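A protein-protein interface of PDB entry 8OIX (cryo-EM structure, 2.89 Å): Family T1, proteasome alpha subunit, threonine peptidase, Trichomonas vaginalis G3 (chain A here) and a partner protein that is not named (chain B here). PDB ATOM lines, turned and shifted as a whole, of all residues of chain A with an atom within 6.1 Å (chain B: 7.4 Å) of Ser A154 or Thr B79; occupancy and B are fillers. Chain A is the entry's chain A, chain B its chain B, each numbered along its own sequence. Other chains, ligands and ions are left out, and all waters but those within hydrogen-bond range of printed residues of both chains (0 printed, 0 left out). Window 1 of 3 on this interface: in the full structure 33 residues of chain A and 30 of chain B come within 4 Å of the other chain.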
ATOM      1  N   VAL A  21       3.466  -5.626 -39.056  1.00  0.00           N
ATOM      2  CA  VAL A  21       4.453  -6.312 -38.227  1.00  0.00           C
ATOM      3  C   VAL A  21       5.054  -7.505 -38.967  1.00  0.00           C
ATOM      4  O   VAL A  21       6.278  -7.689 -38.988  1.00  0.00           O
ATOM      5  CB  VAL A  21       3.812  -6.736 -36.896  1.00  0.00           C
ATOM      6  CG1 VAL A  21       4.748  -7.628 -36.145  1.00  0.00           C
ATOM      7  CG2 VAL A  21       3.468  -5.511 -36.067  1.00  0.00           C
ATOM      8  N   SER A  24       7.374  -6.252 -41.491  1.00  0.00           N
ATOM      9  CA  SER A  24       8.651  -5.885 -40.883  1.00  0.00           C
ATOM     10  C   SER A  24       9.506  -7.113 -40.606  1.00  0.00           C
ATOM     11  O   SER A  24      10.736  -7.050 -40.704  1.00  0.00           O
ATOM     12  CB  SER A  24       8.418  -5.097 -39.594  1.00  0.00           C
ATOM     13  OG  SER A  24       7.663  -5.853 -38.665  1.00  0.00           O
ATOM     14  N   PHE A  25       8.876  -8.240 -40.266  1.00  0.00           N
ATOM     15  CA  PHE A  25       9.621  -9.495 -40.154  1.00  0.00           C
ATOM     16  C   PHE A  25      10.262  -9.865 -41.487  1.00  0.00           C
ATOM     17  O   PHE A  25      11.438 -10.251 -41.549  1.00  0.00           O
ATOM     18  CB  PHE A  25       8.705 -10.625 -39.684  1.00  0.00           C
ATOM     19  CG  PHE A  25       8.515 -10.686 -38.197  1.00  0.00           C
ATOM     20  CD1 PHE A  25       7.844  -9.684 -37.525  1.00  0.00           C
ATOM     21  CD2 PHE A  25       8.997 -11.762 -37.473  1.00  0.00           C
ATOM     22  CE1 PHE A  25       7.662  -9.744 -36.161  1.00  0.00           C
ATOM     23  CE2 PHE A  25       8.817 -11.829 -36.108  1.00  0.00           C
ATOM     24  CZ  PHE A  25       8.147 -10.818 -35.453  1.00  0.00           C
ATOM     25  N   SER A 115      11.321  -3.853 -26.635  1.00  0.00           N
ATOM     26  CA  SER A 115       9.997  -4.414 -26.871  1.00  0.00           C
ATOM     27  C   SER A 115       8.916  -3.355 -26.708  1.00  0.00           C
ATOM     28  O   SER A 115       7.944  -3.325 -27.468  1.00  0.00           O
ATOM     29  CB  SER A 115       9.753  -5.583 -25.919  1.00  0.00           C
ATOM     30  OG  SER A 115       8.432  -6.077 -26.043  1.00  0.00           O
ATOM     31  N   HIS A 118       8.974  -1.313 -29.795  1.00  0.00           N
ATOM     32  CA  HIS A 118       8.364  -2.017 -30.913  1.00  0.00           C
ATOM     33  C   HIS A 118       6.863  -2.168 -30.731  1.00  0.00           C
ATOM     34  O   HIS A 118       6.139  -2.284 -31.724  1.00  0.00           O
ATOM     35  CB  HIS A 118       8.998  -3.395 -31.090  1.00  0.00           C
ATOM     36  CG  HIS A 118      10.362  -3.364 -31.704  1.00  0.00           C
ATOM     37  ND1 HIS A 118      10.759  -2.390 -32.592  1.00  0.00           N
ATOM     38  CD2 HIS A 118      11.418  -4.200 -31.566  1.00  0.00           C
ATOM     39  CE1 HIS A 118      12.004  -2.621 -32.968  1.00  0.00           C
ATOM     40  NE2 HIS A 118      12.427  -3.714 -32.360  1.00  0.00           N
ATOM     41  N   GLN A 119       6.370  -2.039 -29.503  1.00  0.00           N
ATOM     42  CA  GLN A 119       4.937  -2.074 -29.258  1.00  0.00           C
ATOM     43  C   GLN A 119       4.329  -0.720 -29.562  1.00  0.00           C
ATOM     44  O   GLN A 119       3.209  -0.647 -30.081  1.00  0.00           O
ATOM     45  CB  GLN A 119       4.668  -2.478 -27.802  1.00  0.00           C
ATOM     46  CG  GLN A 119       3.208  -2.745 -27.385  1.00  0.00           C
ATOM     47  CD  GLN A 119       2.280  -1.553 -27.501  1.00  0.00           C
ATOM     48  OE1 GLN A 119       2.523  -0.499 -26.918  1.00  0.00           O
ATOM     49  NE2 GLN A 119       1.202  -1.720 -28.252  1.00  0.00           N
ATOM     50  N   SER A 122       4.090  -0.892 -33.232  1.00  0.00           N
ATOM     51  CA  SER A 122       3.002  -1.752 -33.670  1.00  0.00           C
ATOM     52  C   SER A 122       1.631  -1.238 -33.251  1.00  0.00           C
ATOM     53  O   SER A 122       0.621  -1.800 -33.684  1.00  0.00           O
ATOM     54  CB  SER A 122       3.201  -3.171 -33.132  1.00  0.00           C
ATOM     55  OG  SER A 122       2.914  -3.235 -31.747  1.00  0.00           O
ATOM     56  N   PRO A 129       6.761  -0.139 -37.767  1.00  0.00           N
ATOM     57  CA  PRO A 129       7.449  -1.183 -36.995  1.00  0.00           C
ATOM     58  C   PRO A 129       8.901  -1.288 -37.432  1.00  0.00           C
ATOM     59  O   PRO A 129       9.197  -1.575 -38.594  1.00  0.00           O
ATOM     60  CB  PRO A 129       6.656  -2.450 -37.331  1.00  0.00           C
ATOM     61  CG  PRO A 129       5.313  -1.956 -37.739  1.00  0.00           C
ATOM     62  CD  PRO A 129       5.548  -0.648 -38.428  1.00  0.00           C
ATOM     63  N   SER A 130       9.811  -1.046 -36.492  1.00  0.00           N
ATOM     64  CA  SER A 130      11.236  -1.056 -36.804  1.00  0.00           C
ATOM     65  C   SER A 130      11.659  -2.475 -37.150  1.00  0.00           C
ATOM     66  O   SER A 130      11.658  -3.362 -36.290  1.00  0.00           O
ATOM     67  CB  SER A 130      12.044  -0.511 -35.631  1.00  0.00           C
ATOM     68  OG  SER A 130      13.329  -0.093 -36.053  1.00  0.00           O
ATOM     69  N   ILE A 151      14.518  -9.744 -29.430  1.00  0.00           N
ATOM     70  CA  ILE A 151      13.357  -8.882 -29.591  1.00  0.00           C
ATOM     71  C   ILE A 151      13.064  -8.815 -31.082  1.00  0.00           C
ATOM     72  O   ILE A 151      13.867  -8.282 -31.858  1.00  0.00           O
ATOM     73  CB  ILE A 151      13.575  -7.475 -29.015  1.00  0.00           C
ATOM     74  CG1 ILE A 151      14.134  -7.535 -27.592  1.00  0.00           C
ATOM     75  CG2 ILE A 151      12.275  -6.691 -29.036  1.00  0.00           C
ATOM     76  CD1 ILE A 151      15.635  -7.638 -27.523  1.00  0.00           C
ATOM     77  N   GLU A 152      11.931  -9.367 -31.484  1.00  0.00           N
ATOM     78  CA  GLU A 152      11.516  -9.357 -32.875  1.00  0.00           C
ATOM     79  C   GLU A 152      10.885  -8.011 -33.208  1.00  0.00           C
ATOM     80  O   GLU A 152      10.572  -7.224 -32.314  1.00  0.00           O
ATOM     81  CB  GLU A 152      10.556 -10.518 -33.121  1.00  0.00           C
ATOM     82  CG  GLU A 152      11.171 -11.885 -32.884  1.00  0.00           C
ATOM     83  CD  GLU A 152      10.239 -13.018 -33.264  1.00  0.00           C
ATOM     84  OE1 GLU A 152       9.035 -12.934 -32.943  1.00  0.00           O
ATOM     85  OE2 GLU A 152      10.709 -13.993 -33.889  1.00  0.00           O
ATOM     86  N   PRO A 153      10.708  -7.696 -34.497  1.00  0.00           N
ATOM     87  CA  PRO A 153      10.083  -6.409 -34.847  1.00  0.00           C
ATOM     88  C   PRO A 153       8.716  -6.222 -34.221  1.00  0.00           C
ATOM     89  O   PRO A 153       8.296  -5.080 -33.994  1.00  0.00           O
ATOM     90  CB  PRO A 153       9.998  -6.463 -36.377  1.00  0.00           C
ATOM     91  CG  PRO A 153      11.066  -7.388 -36.769  1.00  0.00           C
ATOM     92  CD  PRO A 153      11.146  -8.427 -35.699  1.00  0.00           C
ATOM     93  N   SER A 154       8.005  -7.313 -33.941  1.00  0.00           N
ATOM     94  CA  SER A 154       6.753  -7.233 -33.204  1.00  0.00           C
ATOM     95  C   SER A 154       6.949  -6.745 -31.781  1.00  0.00           C
ATOM     96  O   SER A 154       5.971  -6.348 -31.140  1.00  0.00           O
ATOM     97  CB  SER A 154       6.077  -8.603 -33.169  1.00  0.00           C
ATOM     98  OG  SER A 154       6.903  -9.560 -32.531  1.00  0.00           O
ATOM     99  N   GLY A 155       8.183  -6.745 -31.285  1.00  0.00           N
ATOM    100  CA  GLY A 155       8.445  -6.542 -29.882  1.00  0.00           C
ATOM    101  C   GLY A 155       8.415  -7.805 -29.061  1.00  0.00           C
ATOM    102  O   GLY A 155       8.650  -7.742 -27.849  1.00  0.00           O
ATOM    103  N   TYR A 156       8.123  -8.945 -29.674  1.00  0.00           N
ATOM    104  CA  TYR A 156       8.054 -10.204 -28.944  1.00  0.00           C
ATOM    105  C   TYR A 156       9.454 -10.534 -28.457  1.00  0.00           C
ATOM    106  O   TYR A 156      10.302 -11.005 -29.217  1.00  0.00           O
ATOM    107  CB  TYR A 156       7.491 -11.305 -29.833  1.00  0.00           C
ATOM    108  CG  TYR A 156       7.186 -12.593 -29.107  1.00  0.00           C
ATOM    109  CD1 TYR A 156       6.454 -12.591 -27.927  1.00  0.00           C
ATOM    110  CD2 TYR A 156       7.616 -13.813 -29.608  1.00  0.00           C
ATOM    111  CE1 TYR A 156       6.169 -13.767 -27.261  1.00  0.00           C
ATOM    112  CE2 TYR A 156       7.332 -14.993 -28.951  1.00  0.00           C
ATOM    113  CZ  TYR A 156       6.610 -14.965 -27.778  1.00  0.00           C
ATOM    114  OH  TYR A 156       6.330 -16.141 -27.120  1.00  0.00           O
ATOM    115  N   SER A 157       9.698 -10.281 -27.177  1.00  0.00           N
ATOM    116  CA  SER A 157      11.015 -10.417 -26.581  1.00  0.00           C
ATOM    117  C   SER A 157      11.041 -11.648 -25.691  1.00  0.00           C
ATOM    118  O   SER A 157      10.109 -11.889 -24.918  1.00  0.00           O
ATOM    119  CB  SER A 157      11.385  -9.172 -25.771  1.00  0.00           C
ATOM    120  OG  SER A 157      12.573  -9.380 -25.032  1.00  0.00           O
ATOM    121  N   ASN B  60       9.600 -14.244 -20.272  1.00  0.00           N
ATOM    122  CA  ASN B  60       8.377 -13.764 -20.913  1.00  0.00           C
ATOM    123  C   ASN B  60       7.158 -14.447 -20.298  1.00  0.00           C
ATOM    124  O   ASN B  60       6.287 -14.965 -20.998  1.00  0.00           O
ATOM    125  CB  ASN B  60       8.431 -13.974 -22.425  1.00  0.00           C
ATOM    126  CG  ASN B  60       7.411 -13.127 -23.174  1.00  0.00           C
ATOM    127  OD1 ASN B  60       6.331 -12.829 -22.667  1.00  0.00           O
ATOM    128  ND2 ASN B  60       7.760 -12.730 -24.393  1.00  0.00           N
ATOM    129  N   TYR B  74      -3.108 -13.005 -19.988  1.00  0.00           N
ATOM    130  CA  TYR B  74      -3.629 -12.374 -21.188  1.00  0.00           C
ATOM    131  C   TYR B  74      -3.737 -13.393 -22.307  1.00  0.00           C
ATOM    132  O   TYR B  74      -3.207 -14.504 -22.232  1.00  0.00           O
ATOM    133  CB  TYR B  74      -2.738 -11.228 -21.665  1.00  0.00           C
ATOM    134  CG  TYR B  74      -1.554 -11.721 -22.458  1.00  0.00           C
ATOM    135  CD1 TYR B  74      -0.484 -12.331 -21.827  1.00  0.00           C
ATOM    136  CD2 TYR B  74      -1.513 -11.591 -23.840  1.00  0.00           C
ATOM    137  CE1 TYR B  74       0.596 -12.787 -22.544  1.00  0.00           C
ATOM    138  CE2 TYR B  74      -0.435 -12.049 -24.565  1.00  0.00           C
ATOM    139  CZ  TYR B  74       0.616 -12.647 -23.911  1.00  0.00           C
ATOM    140  OH  TYR B  74       1.696 -13.108 -24.624  1.00  0.00           O
ATOM    141  N   GLY B  76      -3.412 -12.684 -26.623  1.00  0.00           N
ATOM    142  CA  GLY B  76      -3.299 -11.714 -27.692  1.00  0.00           C
ATOM    143  C   GLY B  76      -1.875 -11.272 -27.954  1.00  0.00           C
ATOM    144  O   GLY B  76      -0.933 -12.049 -27.772  1.00  0.00           O
ATOM    145  N   VAL B  77      -1.708 -10.026 -28.391  1.00  0.00           N
ATOM    146  CA  VAL B  77      -0.382  -9.499 -28.696  1.00  0.00           C
ATOM    147  C   VAL B  77       0.420  -9.400 -27.406  1.00  0.00           C
ATOM    148  O   VAL B  77       0.072  -8.637 -26.499  1.00  0.00           O
ATOM    149  CB  VAL B  77      -0.480  -8.140 -29.398  1.00  0.00           C
ATOM    150  CG1 VAL B  77       0.904  -7.592 -29.685  1.00  0.00           C
ATOM    151  CG2 VAL B  77      -1.277  -8.269 -30.681  1.00  0.00           C
ATOM    152  N   ASN B  78       1.521 -10.147 -27.335  1.00  0.00           N
ATOM    153  CA  ASN B  78       2.306 -10.202 -26.106  1.00  0.00           C
ATOM    154  C   ASN B  78       2.791  -8.819 -25.691  1.00  0.00           C
ATOM    155  O   ASN B  78       2.768  -8.472 -24.504  1.00  0.00           O
ATOM    156  CB  ASN B  78       3.483 -11.159 -26.294  1.00  0.00           C
ATOM    157  CG  ASN B  78       4.436 -11.147 -25.123  1.00  0.00           C
ATOM    158  OD1 ASN B  78       5.563 -10.668 -25.231  1.00  0.00           O
ATOM    159  ND2 ASN B  78       3.986 -11.673 -23.990  1.00  0.00           N
ATOM    160  N   THR B  79       3.232  -8.013 -26.657  1.00  0.00           N
ATOM    161  CA  THR B  79       3.755  -6.689 -26.344  1.00  0.00           C
ATOM    162  C   THR B  79       2.666  -5.762 -25.821  1.00  0.00           C
ATOM    163  O   THR B  79       2.916  -4.944 -24.926  1.00  0.00           O
ATOM    164  CB  THR B  79       4.413  -6.099 -27.583  1.00  0.00           C
ATOM    165  OG1 THR B  79       3.409  -5.818 -28.565  1.00  0.00           O
ATOM    166  CG2 THR B  79       5.367  -7.101 -28.154  1.00  0.00           C
ATOM    167  N   ASP B  80       1.456  -5.859 -26.376  1.00  0.00           N
ATOM    168  CA  ASP B  80       0.348  -5.072 -25.849  1.00  0.00           C
ATOM    169  C   ASP B  80       0.053  -5.455 -24.406  1.00  0.00           C
ATOM    170  O   ASP B  80      -0.221  -4.588 -23.567  1.00  0.00           O
ATOM    171  CB  ASP B  80      -0.896  -5.256 -26.717  1.00  0.00           C
ATOM    172  CG  ASP B  80      -0.725  -4.686 -28.107  1.00  0.00           C
ATOM    173  OD1 ASP B  80       0.381  -4.198 -28.420  1.00  0.00           O
ATOM    174  OD2 ASP B  80      -1.699  -4.721 -28.886  1.00  0.00           O
ATOM    175  N   PHE B  81       0.116  -6.752 -24.097  1.00  0.00           N
ATOM    176  CA  PHE B  81      -0.052  -7.176 -22.715  1.00  0.00           C
ATOM    177  C   PHE B  81       1.045  -6.617 -21.830  1.00  0.00           C
ATOM    178  O   PHE B  81       0.785  -6.234 -20.690  1.00  0.00           O
ATOM    179  CB  PHE B  81      -0.064  -8.694 -22.596  1.00  0.00           C
ATOM    180  CG  PHE B  81       0.210  -9.180 -21.200  1.00  0.00           C
ATOM    181  CD1 PHE B  81      -0.720  -8.990 -20.191  1.00  0.00           C
ATOM    182  CD2 PHE B  81       1.405  -9.803 -20.888  1.00  0.00           C
ATOM    183  CE1 PHE B  81      -0.474  -9.429 -18.908  1.00  0.00           C
ATOM    184  CE2 PHE B  81       1.656 -10.246 -19.605  1.00  0.00           C
ATOM    185  CZ  PHE B  81       0.716 -10.056 -18.614  1.00  0.00           C
ATOM    186  N   HIS B  82       2.285  -6.600 -22.316  1.00  0.00           N
ATOM    187  CA  HIS B  82       3.368  -6.072 -21.495  1.00  0.00           C
ATOM    188  C   HIS B  82       3.180  -4.585 -21.226  1.00  0.00           C
ATOM    189  O   HIS B  82       3.433  -4.112 -20.113  1.00  0.00           O
ATOM    190  CB  HIS B  82       4.717  -6.334 -22.159  1.00  0.00           C
ATOM    191  CG  HIS B  82       5.136  -7.768 -22.115  1.00  0.00           C
ATOM    192  ND1 HIS B  82       5.171  -8.496 -20.947  1.00  0.00           N
ATOM    193  CD2 HIS B  82       5.546  -8.607 -23.094  1.00  0.00           C
ATOM    194  CE1 HIS B  82       5.579  -9.725 -21.208  1.00  0.00           C
ATOM    195  NE2 HIS B  82       5.814  -9.819 -22.504  1.00  0.00           N
ATOM    196  N   VAL B  83       2.729  -3.834 -22.231  1.00  0.00           N
ATOM    197  CA  VAL B  83       2.479  -2.409 -22.033  1.00  0.00           C
ATOM    198  C   VAL B  83       1.351  -2.201 -21.027  1.00  0.00           C
ATOM    199  O   VAL B  83       1.460  -1.384 -20.103  1.00  0.00           O
ATOM    200  CB  VAL B  83       2.183  -1.723 -23.380  1.00  0.00           C
ATOM    201  CG1 VAL B  83       1.136  -0.631 -23.221  1.00  0.00           C
ATOM    202  CG2 VAL B  83       3.463  -1.157 -23.964  1.00  0.00           C
ATOM    203  N   ILE B  84       0.257  -2.952 -21.180  1.00  0.00           N
ATOM    204  CA  ILE B  84      -0.861  -2.829 -20.246  1.00  0.00           C
ATOM    205  C   ILE B  84      -0.439  -3.263 -18.850  1.00  0.00           C
ATOM    206  O   ILE B  84      -0.887  -2.702 -17.849  1.00  0.00           O
ATOM    207  CB  ILE B  84      -2.078  -3.626 -20.744  1.00  0.00           C
ATOM    208  CG1 ILE B  84      -2.680  -2.957 -21.973  1.00  0.00           C
ATOM    209  CG2 ILE B  84      -3.129  -3.747 -19.658  1.00  0.00           C
ATOM    210  CD1 ILE B  84      -3.607  -3.847 -22.721  1.00  0.00           C
ATOM    211  N   LEU B  85       0.427  -4.271 -18.763  1.00  0.00           N
ATOM    212  CA  LEU B  85       0.896  -4.758 -17.473  1.00  0.00           C
ATOM    213  C   LEU B  85       1.766  -3.724 -16.776  1.00  0.00           C
ATOM    214  O   LEU B  85       1.629  -3.509 -15.568  1.00  0.00           O
ATOM    215  CB  LEU B  85       1.667  -6.058 -17.675  1.00  0.00           C
ATOM    216  CG  LEU B  85       2.432  -6.609 -16.480  1.00  0.00           C
ATOM    217  CD1 LEU B  85       1.490  -7.189 -15.450  1.00  0.00           C
ATOM    218  CD2 LEU B  85       3.421  -7.645 -16.965  1.00  0.00           C
ATOM    219  N   ARG B 126      -4.167   1.808 -32.488  1.00  0.00           N
ATOM    220  CA  ARG B 126      -5.077   0.684 -32.577  1.00  0.00           C
ATOM    221  C   ARG B 126      -5.432   0.195 -31.180  1.00  0.00           C
ATOM    222  O   ARG B 126      -4.683   0.425 -30.224  1.00  0.00           O
ATOM    223  CB  ARG B 126      -4.440  -0.464 -33.371  1.00  0.00           C
ATOM    224  CG  ARG B 126      -3.077  -0.863 -32.853  1.00  0.00           C
ATOM    225  CD  ARG B 126      -2.713  -2.266 -33.279  1.00  0.00           C
ATOM    226  NE  ARG B 126      -1.451  -2.701 -32.693  1.00  0.00           N
ATOM    227  CZ  ARG B 126      -1.318  -3.158 -31.457  1.00  0.00           C
ATOM    228  NH1 ARG B 126      -2.349  -3.238 -30.634  1.00  0.00           N
ATOM    229  NH2 ARG B 126      -0.118  -3.542 -31.033  1.00  0.00           N
ATOM    230  N   PHE B 128      -5.652  -2.276 -28.034  1.00  0.00           N
ATOM    231  CA  PHE B 128      -4.774  -3.335 -27.563  1.00  0.00           C
ATOM    232  C   PHE B 128      -5.340  -4.688 -27.963  1.00  0.00           C
ATOM    233  O   PHE B 128      -6.491  -5.004 -27.662  1.00  0.00           O
ATOM    234  CB  PHE B 128      -4.619  -3.264 -26.048  1.00  0.00           C
ATOM    235  CG  PHE B 128      -3.862  -2.066 -25.567  1.00  0.00           C
ATOM    236  CD1 PHE B 128      -2.481  -2.029 -25.638  1.00  0.00           C
ATOM    237  CD2 PHE B 128      -4.528  -0.984 -25.023  1.00  0.00           C
ATOM    238  CE1 PHE B 128      -1.782  -0.931 -25.186  1.00  0.00           C
ATOM    239  CE2 PHE B 128      -3.833   0.115 -24.569  1.00  0.00           C
ATOM    240  CZ  PHE B 128      -2.458   0.143 -24.652  1.00  0.00           C
ATOM    241  N   VAL B 130      -5.299  -7.632 -26.829  1.00  0.00           N
ATOM    242  CA  VAL B 130      -5.224  -8.606 -25.745  1.00  0.00           C
ATOM    243  C   VAL B 130      -6.520  -8.572 -24.956  1.00  0.00           C
ATOM    244  O   VAL B 130      -7.152  -7.521 -24.816  1.00  0.00           O
ATOM    245  CB  VAL B 130      -4.031  -8.347 -24.803  1.00  0.00           C
ATOM    246  CG1 VAL B 130      -2.737  -8.522 -25.531  1.00  0.00           C
ATOM    247  CG2 VAL B 130      -4.112  -6.957 -24.226  1.00  0.00           C
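The side-chain amide nitrogen of Asn B60 is in hydrogen-bond range of the backbone carbonyl oxygen of Ser A157 (2.5 Å).
The side-chain carboxylate of Asp B80 sits at hydrogen-bond distance from the side-chain amide nitrogen of Gln A119, at 2.6 Å.
O of Ser A122 is in hydrogen-bond range of NE of Arg B126, at 2.5 Å.
The side-chain amide oxygen of Asn B60 lies within hydrogen-bond range of the side-chain amide nitrogen of Asn B78, at 2.9 Å.
The side-chain amide nitrogen (ND2) of Asn B78 sits at hydrogen-bond distance from the side-chain hydroxyl (OH) of Tyr B74.
The backbone carbonyl oxygen of Gly A155 lies within hydrogen-bond range of the side-chain hydroxyl of Ser A115 (2.5 Å).
The backbone carbonyl oxygen of Gln A119 is in hydrogen-bond range of the side-chain hydroxyl of Ser A122, 3.1 Å away.
The side-chain carboxylate (OD1) of Asp B80 lies within hydrogen-bond range of the side-chain hydroxyl (OG1) of Thr B79, 3.4 Å away.
O of His A118 is in hydrogen-bond range of OG of Ser A122 (3.4 Å).
OG of Ser A115 touches CG2 of Thr B79 (3.9 Å).
Thr B79 touches Gln A119 (OG1 to CG, 3.3 Å).
CG2 of Val B83 touches OE1 of Gln A119, 3.2 Å away.
Gln A119 touches Arg B126 (NE2 to NH2, 3.6 Å).
Ser A154 touches Thr B79.
Thr B79 touches Gly A155 (CG2 to C, 3.3 Å).
CE1 of Tyr A156 touches ND2 of Asn B60, at 3.4 Å.
Asn B78 touches Tyr A156.
Tyr A156 touches Thr B79 (N to CG2, 3.6 Å).
Ser A154 touches just one residue of chain B: Thr B79.
Thr B79 touches just these residues of chain A: Ser A115, Gln A119, Ser A154, Gly A155 and Tyr A156.
Of the printed residues of chain B, Ser A157 touches Asn B60 (2.5 Å).
Printed residues of chain B within 4 Å of Gln A119: Thr B79, Asp B80, Val B83 and Arg B126.
Of the printed residues of chain A, Asn B78 touches Tyr A156 (3.4 Å).
Ser A130 touches none of the printed residues of chain B.
The nearest residue of chain A that does not touch Thr B79 is Ser A122 (4.1 Å).
The nearest printed residue of chain B that does not touch Ser A115 is His B82 (4.8 Å).
Printed residues of chain A that touch a printed residue of chain B: Ser A115, Gln A119, Ser A122, Ser A154, Gly A155, Tyr A156 and Ser A157.
Hydrophobic or aromatic side chains of chain A within 4 Å of the printed part of chain B: Tyr A156.
Of the 15 printed residues of chain B, 6 touch a printed residue of chain A.
Printed residues of chain B that touch a printed residue of chain A: Asn B60, Asn B78, Thr B79, Asp B80, Val B83 and Arg B126.
Hydrophobic or aromatic side chains of chain B that line the printed part of chain A: Val B83.
Among the printed residues, 12 pairs touch across the chains.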
